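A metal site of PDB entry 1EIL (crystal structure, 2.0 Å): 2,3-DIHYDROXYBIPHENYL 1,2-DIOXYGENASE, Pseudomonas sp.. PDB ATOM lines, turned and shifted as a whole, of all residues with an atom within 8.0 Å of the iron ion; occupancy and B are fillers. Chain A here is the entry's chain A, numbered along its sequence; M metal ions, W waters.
A ring nitrogen (NE2) of His 240 lies within hydrogen-bond range of the side-chain hydroxyl of Tyr 249 (2.7 Å).
The side-chain carboxylate of Glu 260 lies within hydrogen-bond range of the side-chain hydroxyl of Tyr 249 (3.2 Å).
The backbone NH (N) of Met 211 lies within hydrogen-bond range of the backbone carbonyl oxygen (O) of His 145 (2.7 Å).
A ring nitrogen (ND1) of His 208 lies within hydrogen-bond range of a ring nitrogen (ND1) of His 209 (2.7 Å).
The side-chain carboxylate (OE2) of Glu 260 lies within hydrogen-bond range of a ring nitrogen (NE2) of His 240 (3.2 Å).
The backbone carbonyl oxygen of Glu 260 lies within hydrogen-bond range of the backbone NH of Leu 212, at 3.0 Å.
The backbone carbonyl oxygen (O) of Phe 210 sits at hydrogen-bond distance from the backbone NH (N) of Glu 260 (2.9 Å).
O of His 209 lies within hydrogen-bond range of N of Val 147, at 3.2 Å.
Tyr 249 touches the iron ion (OH to FE, 3.7 Å).
Water W1 binds the iron ion.
The iron ion is bound by the side-chain carboxylate (OE1) of Glu 260 (2.1 Å).
The iron ion is bound by NE2 of His 145 (2.2 Å).
NE2 of His 209 binds the iron ion, at 2.3 Å.
Water W2 is bound to the iron ion.
Water W2 lies within hydrogen-bond range of the side-chain carboxylate (OE2) of Glu 260 and the side-chain carboxylate (OD1) of Asp 243.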
ATOM      1  N   HIS A 145      10.969 -21.937  -9.948  1.00  0.00           N
ATOM      2  CA  HIS A 145       9.868 -21.449 -10.769  1.00  0.00           C
ATOM      3  C   HIS A 145       9.708 -19.940 -10.670  1.00  0.00           C
ATOM      4  O   HIS A 145      10.370 -19.286  -9.863  1.00  0.00           O
ATOM      5  CB  HIS A 145       8.540 -22.141 -10.381  1.00  0.00           C
ATOM      6  CG  HIS A 145       7.931 -21.666  -9.094  1.00  0.00           C
ATOM      7  ND1 HIS A 145       7.693 -22.509  -8.034  1.00  0.00           N
ATOM      8  CD2 HIS A 145       7.494 -20.446  -8.702  1.00  0.00           C
ATOM      9  CE1 HIS A 145       7.132 -21.827  -7.043  1.00  0.00           C
ATOM     10  NE2 HIS A 145       7.002 -20.574  -7.423  1.00  0.00           N
ATOM     11  N   PHE A 146       8.851 -19.381 -11.526  1.00  0.00           N
ATOM     12  CA  PHE A 146       8.576 -17.959 -11.486  1.00  0.00           C
ATOM     13  C   PHE A 146       7.181 -17.690 -12.012  1.00  0.00           C
ATOM     14  O   PHE A 146       6.650 -18.449 -12.818  1.00  0.00           O
ATOM     15  CB  PHE A 146       9.621 -17.146 -12.269  1.00  0.00           C
ATOM     16  CG  PHE A 146       9.601 -17.331 -13.775  1.00  0.00           C
ATOM     17  CD1 PHE A 146       8.780 -16.555 -14.576  1.00  0.00           C
ATOM     18  CD2 PHE A 146      10.480 -18.228 -14.381  1.00  0.00           C
ATOM     19  CE1 PHE A 146       8.823 -16.653 -15.965  1.00  0.00           C
ATOM     20  CE2 PHE A 146      10.543 -18.327 -15.777  1.00  0.00           C
ATOM     21  CZ  PHE A 146       9.715 -17.533 -16.563  1.00  0.00           C
ATOM     22  N   VAL A 147       6.595 -16.616 -11.496  1.00  0.00           N
ATOM     23  CA  VAL A 147       5.257 -16.207 -11.877  1.00  0.00           C
ATOM     24  C   VAL A 147       5.386 -15.092 -12.896  1.00  0.00           C
ATOM     25  O   VAL A 147       5.927 -14.025 -12.595  1.00  0.00           O
ATOM     26  CB  VAL A 147       4.477 -15.714 -10.673  1.00  0.00           C
ATOM     27  CG1 VAL A 147       3.109 -15.243 -11.111  1.00  0.00           C
ATOM     28  CG2 VAL A 147       4.379 -16.834  -9.632  1.00  0.00           C
ATOM     29  N   PHE A 186      -1.092 -22.138 -13.049  1.00  0.00           N
ATOM     30  CA  PHE A 186       0.161 -22.782 -12.721  1.00  0.00           C
ATOM     31  C   PHE A 186       0.501 -23.925 -13.674  1.00  0.00           C
ATOM     32  O   PHE A 186      -0.246 -24.898 -13.787  1.00  0.00           O
ATOM     33  CB  PHE A 186       0.084 -23.294 -11.273  1.00  0.00           C
ATOM     34  CG  PHE A 186      -0.126 -22.192 -10.269  1.00  0.00           C
ATOM     35  CD1 PHE A 186      -1.410 -21.686 -10.035  1.00  0.00           C
ATOM     36  CD2 PHE A 186       0.946 -21.647  -9.577  1.00  0.00           C
ATOM     37  CE1 PHE A 186      -1.618 -20.639  -9.132  1.00  0.00           C
ATOM     38  CE2 PHE A 186       0.749 -20.607  -8.667  1.00  0.00           C
ATOM     39  CZ  PHE A 186      -0.530 -20.105  -8.446  1.00  0.00           C
ATOM     40  N   HIS A 194       4.877 -26.550 -10.443  1.00  0.00           N
ATOM     41  CA  HIS A 194       4.875 -25.583 -11.523  1.00  0.00           C
ATOM     42  C   HIS A 194       6.230 -24.947 -11.673  1.00  0.00           C
ATOM     43  O   HIS A 194       6.947 -24.727 -10.699  1.00  0.00           O
ATOM     44  CB  HIS A 194       3.775 -24.524 -11.357  1.00  0.00           C
ATOM     45  CG  HIS A 194       3.994 -23.560 -10.235  1.00  0.00           C
ATOM     46  ND1 HIS A 194       3.598 -23.817  -8.946  1.00  0.00           N
ATOM     47  CD2 HIS A 194       4.495 -22.303 -10.238  1.00  0.00           C
ATOM     48  CE1 HIS A 194       3.846 -22.769  -8.192  1.00  0.00           C
ATOM     49  NE2 HIS A 194       4.393 -21.834  -8.948  1.00  0.00           N
ATOM     50  N   ALA A 197       4.058 -19.871 -13.851  1.00  0.00           N
ATOM     51  CA  ALA A 197       2.658 -19.570 -13.542  1.00  0.00           C
ATOM     52  C   ALA A 197       2.336 -18.285 -14.290  1.00  0.00           C
ATOM     53  O   ALA A 197       3.192 -17.421 -14.401  1.00  0.00           O
ATOM     54  CB  ALA A 197       2.454 -19.376 -12.051  1.00  0.00           C
ATOM     55  N   HIS A 208       6.489 -11.572 -10.962  1.00  0.00           N
ATOM     56  CA  HIS A 208       6.144 -11.172  -9.605  1.00  0.00           C
ATOM     57  C   HIS A 208       7.282 -11.628  -8.676  1.00  0.00           C
ATOM     58  O   HIS A 208       7.793 -10.857  -7.873  1.00  0.00           O
ATOM     59  CB  HIS A 208       4.822 -11.818  -9.182  1.00  0.00           C
ATOM     60  CG  HIS A 208       4.511 -11.655  -7.726  1.00  0.00           C
ATOM     61  ND1 HIS A 208       4.868 -12.593  -6.781  1.00  0.00           N
ATOM     62  CD2 HIS A 208       3.889 -10.653  -7.049  1.00  0.00           C
ATOM     63  CE1 HIS A 208       4.489 -12.173  -5.581  1.00  0.00           C
ATOM     64  NE2 HIS A 208       3.900 -10.994  -5.725  1.00  0.00           N
ATOM     65  N   HIS A 209       7.679 -12.885  -8.808  1.00  0.00           N
ATOM     66  CA  HIS A 209       8.757 -13.443  -7.998  1.00  0.00           C
ATOM     67  C   HIS A 209       9.339 -14.701  -8.638  1.00  0.00           C
ATOM     68  O   HIS A 209       8.741 -15.273  -9.549  1.00  0.00           O
ATOM     69  CB  HIS A 209       8.246 -13.809  -6.591  1.00  0.00           C
ATOM     70  CG  HIS A 209       7.401 -15.051  -6.567  1.00  0.00           C
ATOM     71  ND1 HIS A 209       6.024 -15.022  -6.694  1.00  0.00           N
ATOM     72  CD2 HIS A 209       7.735 -16.354  -6.423  1.00  0.00           C
ATOM     73  CE1 HIS A 209       5.548 -16.255  -6.634  1.00  0.00           C
ATOM     74  NE2 HIS A 209       6.570 -17.087  -6.467  1.00  0.00           N
ATOM     75  N   PHE A 210      10.518 -15.112  -8.178  1.00  0.00           N
ATOM     76  CA  PHE A 210      11.086 -16.369  -8.624  1.00  0.00           C
ATOM     77  C   PHE A 210      11.232 -17.174  -7.339  1.00  0.00           C
ATOM     78  O   PHE A 210      11.326 -16.595  -6.253  1.00  0.00           O
ATOM     79  CB  PHE A 210      12.438 -16.190  -9.359  1.00  0.00           C
ATOM     80  CG  PHE A 210      13.562 -15.690  -8.520  1.00  0.00           C
ATOM     81  CD1 PHE A 210      14.581 -16.548  -8.114  1.00  0.00           C
ATOM     82  CD2 PHE A 210      13.678 -14.336  -8.217  1.00  0.00           C
ATOM     83  CE1 PHE A 210      15.694 -16.065  -7.441  1.00  0.00           C
ATOM     84  CE2 PHE A 210      14.785 -13.849  -7.532  1.00  0.00           C
ATOM     85  CZ  PHE A 210      15.802 -14.719  -7.146  1.00  0.00           C
ATOM     86  N   MET A 211      11.192 -18.501  -7.452  1.00  0.00           N
ATOM     87  CA  MET A 211      11.270 -19.354  -6.267  1.00  0.00           C
ATOM     88  C   MET A 211      12.421 -20.349  -6.272  1.00  0.00           C
ATOM     89  O   MET A 211      12.740 -20.921  -7.303  1.00  0.00           O
ATOM     90  CB  MET A 211       9.946 -20.115  -6.119  1.00  0.00           C
ATOM     91  CG  MET A 211       9.825 -20.968  -4.863  1.00  0.00           C
ATOM     92  SD  MET A 211      10.470 -22.647  -5.106  1.00  0.00           S
ATOM     93  CE  MET A 211      10.109 -23.384  -3.492  1.00  0.00           C
ATOM     94  N   LEU A 212      13.042 -20.526  -5.103  1.00  0.00           N
ATOM     95  CA  LEU A 212      14.122 -21.487  -4.926  1.00  0.00           C
ATOM     96  C   LEU A 212      13.670 -22.429  -3.801  1.00  0.00           C
ATOM     97  O   LEU A 212      13.060 -21.988  -2.822  1.00  0.00           O
ATOM     98  CB  LEU A 212      15.441 -20.812  -4.536  1.00  0.00           C
ATOM     99  CG  LEU A 212      16.165 -19.925  -5.571  1.00  0.00           C
ATOM    100  CD1 LEU A 212      17.354 -19.289  -4.894  1.00  0.00           C
ATOM    101  CD2 LEU A 212      16.636 -20.744  -6.770  1.00  0.00           C
ATOM    102  N   HIS A 240       1.426 -22.973   0.658  1.00  0.00           N
ATOM    103  CA  HIS A 240       0.477 -22.752  -0.428  1.00  0.00           C
ATOM    104  C   HIS A 240      -0.571 -23.857  -0.549  1.00  0.00           C
ATOM    105  O   HIS A 240      -0.309 -25.005  -0.197  1.00  0.00           O
ATOM    106  CB  HIS A 240       1.232 -22.601  -1.743  1.00  0.00           C
ATOM    107  CG  HIS A 240       1.892 -21.277  -1.901  1.00  0.00           C
ATOM    108  ND1 HIS A 240       1.184 -20.089  -1.946  1.00  0.00           N
ATOM    109  CD2 HIS A 240       3.202 -20.929  -2.007  1.00  0.00           C
ATOM    110  CE1 HIS A 240       2.030 -19.078  -2.069  1.00  0.00           C
ATOM    111  NE2 HIS A 240       3.253 -19.555  -2.112  1.00  0.00           N
ATOM    112  N   ASN A 242      -2.072 -25.060  -3.452  1.00  0.00           N
ATOM    113  CA  ASN A 242      -1.852 -26.010  -4.527  1.00  0.00           C
ATOM    114  C   ASN A 242      -0.595 -26.869  -4.518  1.00  0.00           C
ATOM    115  O   ASN A 242      -0.695 -28.089  -4.643  1.00  0.00           O
ATOM    116  CB  ASN A 242      -2.001 -25.328  -5.909  1.00  0.00           C
ATOM    117  CG  ASN A 242      -1.105 -24.116  -6.077  1.00  0.00           C
ATOM    118  OD1 ASN A 242      -0.487 -23.648  -5.131  1.00  0.00           O
ATOM    119  ND2 ASN A 242      -1.049 -23.596  -7.298  1.00  0.00           N
ATOM    120  N   ASP A 243       0.595 -26.274  -4.371  1.00  0.00           N
ATOM    121  CA  ASP A 243       1.808 -27.083  -4.364  1.00  0.00           C
ATOM    122  C   ASP A 243       2.289 -27.415  -2.970  1.00  0.00           C
ATOM    123  O   ASP A 243       3.159 -28.270  -2.802  1.00  0.00           O
ATOM    124  CB  ASP A 243       2.927 -26.399  -5.162  1.00  0.00           C
ATOM    125  CG  ASP A 243       3.389 -25.081  -4.537  1.00  0.00           C
ATOM    126  OD1 ASP A 243       4.400 -24.530  -5.024  1.00  0.00           O
ATOM    127  OD2 ASP A 243       2.744 -24.608  -3.576  1.00  0.00           O
ATOM    128  N   THR A 245       4.054 -25.646  -1.008  1.00  0.00           N
ATOM    129  CA  THR A 245       5.402 -25.152  -0.762  1.00  0.00           C
ATOM    130  C   THR A 245       5.319 -24.376   0.546  1.00  0.00           C
ATOM    131  O   THR A 245       4.455 -23.501   0.693  1.00  0.00           O
ATOM    132  CB  THR A 245       5.853 -24.175  -1.884  1.00  0.00           C
ATOM    133  OG1 THR A 245       6.306 -24.930  -3.007  1.00  0.00           O
ATOM    134  CG2 THR A 245       6.992 -23.277  -1.425  1.00  0.00           C
ATOM    135  N   SER A 247       6.908 -21.691   2.588  1.00  0.00           N
ATOM    136  CA  SER A 247       7.865 -20.631   2.310  1.00  0.00           C
ATOM    137  C   SER A 247       7.502 -19.245   2.846  1.00  0.00           C
ATOM    138  O   SER A 247       6.492 -19.052   3.519  1.00  0.00           O
ATOM    139  CB  SER A 247       8.002 -20.490   0.793  1.00  0.00           C
ATOM    140  OG  SER A 247       6.778 -19.974   0.264  1.00  0.00           O
ATOM    141  N   TYR A 249       8.184 -14.877   1.545  1.00  0.00           N
ATOM    142  CA  TYR A 249       8.594 -14.039   0.421  1.00  0.00           C
ATOM    143  C   TYR A 249       9.411 -12.889   0.952  1.00  0.00           C
ATOM    144  O   TYR A 249       9.276 -12.516   2.116  1.00  0.00           O
ATOM    145  CB  TYR A 249       7.378 -13.497  -0.328  1.00  0.00           C
ATOM    146  CG  TYR A 249       6.622 -14.550  -1.098  1.00  0.00           C
ATOM    147  CD1 TYR A 249       6.707 -14.626  -2.477  1.00  0.00           C
ATOM    148  CD2 TYR A 249       5.791 -15.446  -0.431  1.00  0.00           C
ATOM    149  CE1 TYR A 249       5.983 -15.564  -3.191  1.00  0.00           C
ATOM    150  CE2 TYR A 249       5.051 -16.397  -1.132  1.00  0.00           C
ATOM    151  CZ  TYR A 249       5.155 -16.449  -2.503  1.00  0.00           C
ATOM    152  OH  TYR A 249       4.426 -17.383  -3.205  1.00  0.00           O
ATOM    153  N   VAL A 259      11.448 -12.614  -4.066  1.00  0.00           N
ATOM    154  CA  VAL A 259      12.009 -13.952  -4.089  1.00  0.00           C
ATOM    155  C   VAL A 259      11.206 -14.794  -3.109  1.00  0.00           C
ATOM    156  O   VAL A 259      10.716 -14.294  -2.076  1.00  0.00           O
ATOM    157  CB  VAL A 259      13.493 -13.979  -3.679  1.00  0.00           C
ATOM    158  CG1 VAL A 259      13.663 -13.548  -2.233  1.00  0.00           C
ATOM    159  CG2 VAL A 259      14.048 -15.362  -3.872  1.00  0.00           C
ATOM    160  N   GLU A 260      11.024 -16.062  -3.435  1.00  0.00           N
ATOM    161  CA  GLU A 260      10.316 -16.958  -2.542  1.00  0.00           C
ATOM    162  C   GLU A 260      11.316 -18.042  -2.165  1.00  0.00           C
ATOM    163  O   GLU A 260      11.985 -18.593  -3.027  1.00  0.00           O
ATOM    164  CB  GLU A 260       9.102 -17.558  -3.250  1.00  0.00           C
ATOM    165  CG  GLU A 260       8.303 -18.479  -2.354  1.00  0.00           C
ATOM    166  CD  GLU A 260       7.210 -19.203  -3.091  1.00  0.00           C
ATOM    167  OE1 GLU A 260       7.192 -19.146  -4.340  1.00  0.00           O
ATOM    168  OE2 GLU A 260       6.377 -19.838  -2.415  1.00  0.00           O
ATOM    169  N   PHE A 261      11.422 -18.315  -0.873  1.00  0.00           N
ATOM    170  CA  PHE A 261      12.348 -19.333  -0.372  1.00  0.00           C
ATOM    171  C   PHE A 261      11.474 -20.391   0.291  1.00  0.00           C
ATOM    172  O   PHE A 261      10.823 -20.111   1.306  1.00  0.00           O
ATOM    173  CB  PHE A 261      13.306 -18.682   0.629  1.00  0.00           C
ATOM    174  CG  PHE A 261      14.605 -19.424   0.817  1.00  0.00           C
ATOM    175  CD1 PHE A 261      15.756 -19.008   0.168  1.00  0.00           C
ATOM    176  CD2 PHE A 261      14.681 -20.526   1.660  1.00  0.00           C
ATOM    177  CE1 PHE A 261      16.967 -19.659   0.361  1.00  0.00           C
ATOM    178  CE2 PHE A 261      15.871 -21.199   1.867  1.00  0.00           C
ATOM    179  CZ  PHE A 261      17.030 -20.764   1.208  1.00  0.00           C
ATOM    180  N   HIS A 285       1.539 -17.068   5.570  1.00  0.00           N
ATOM    181  CA  HIS A 285       1.775 -16.169   4.442  1.00  0.00           C
ATOM    182  C   HIS A 285       1.151 -14.789   4.657  1.00  0.00           C
ATOM    183  O   HIS A 285       0.820 -14.104   3.687  1.00  0.00           O
ATOM    184  CB  HIS A 285       1.215 -16.770   3.148  1.00  0.00           C
ATOM    185  CG  HIS A 285       2.172 -17.687   2.453  1.00  0.00           C
ATOM    186  ND1 HIS A 285       3.546 -17.605   2.614  1.00  0.00           N
ATOM    187  CD2 HIS A 285       1.961 -18.708   1.585  1.00  0.00           C
ATOM    188  CE1 HIS A 285       4.134 -18.532   1.883  1.00  0.00           C
ATOM    189  NE2 HIS A 285       3.203 -19.219   1.249  1.00  0.00           N
HETATM  190 FE    FE M   1       5.917 -19.238  -5.992  1.00  0.00          FE
HETATM  191  O   HOH W   1       4.216 -19.397  -7.029  1.00  0.00           O
HETATM  192  O   HOH W   2       5.170 -21.167  -4.749  1.00  0.00           O
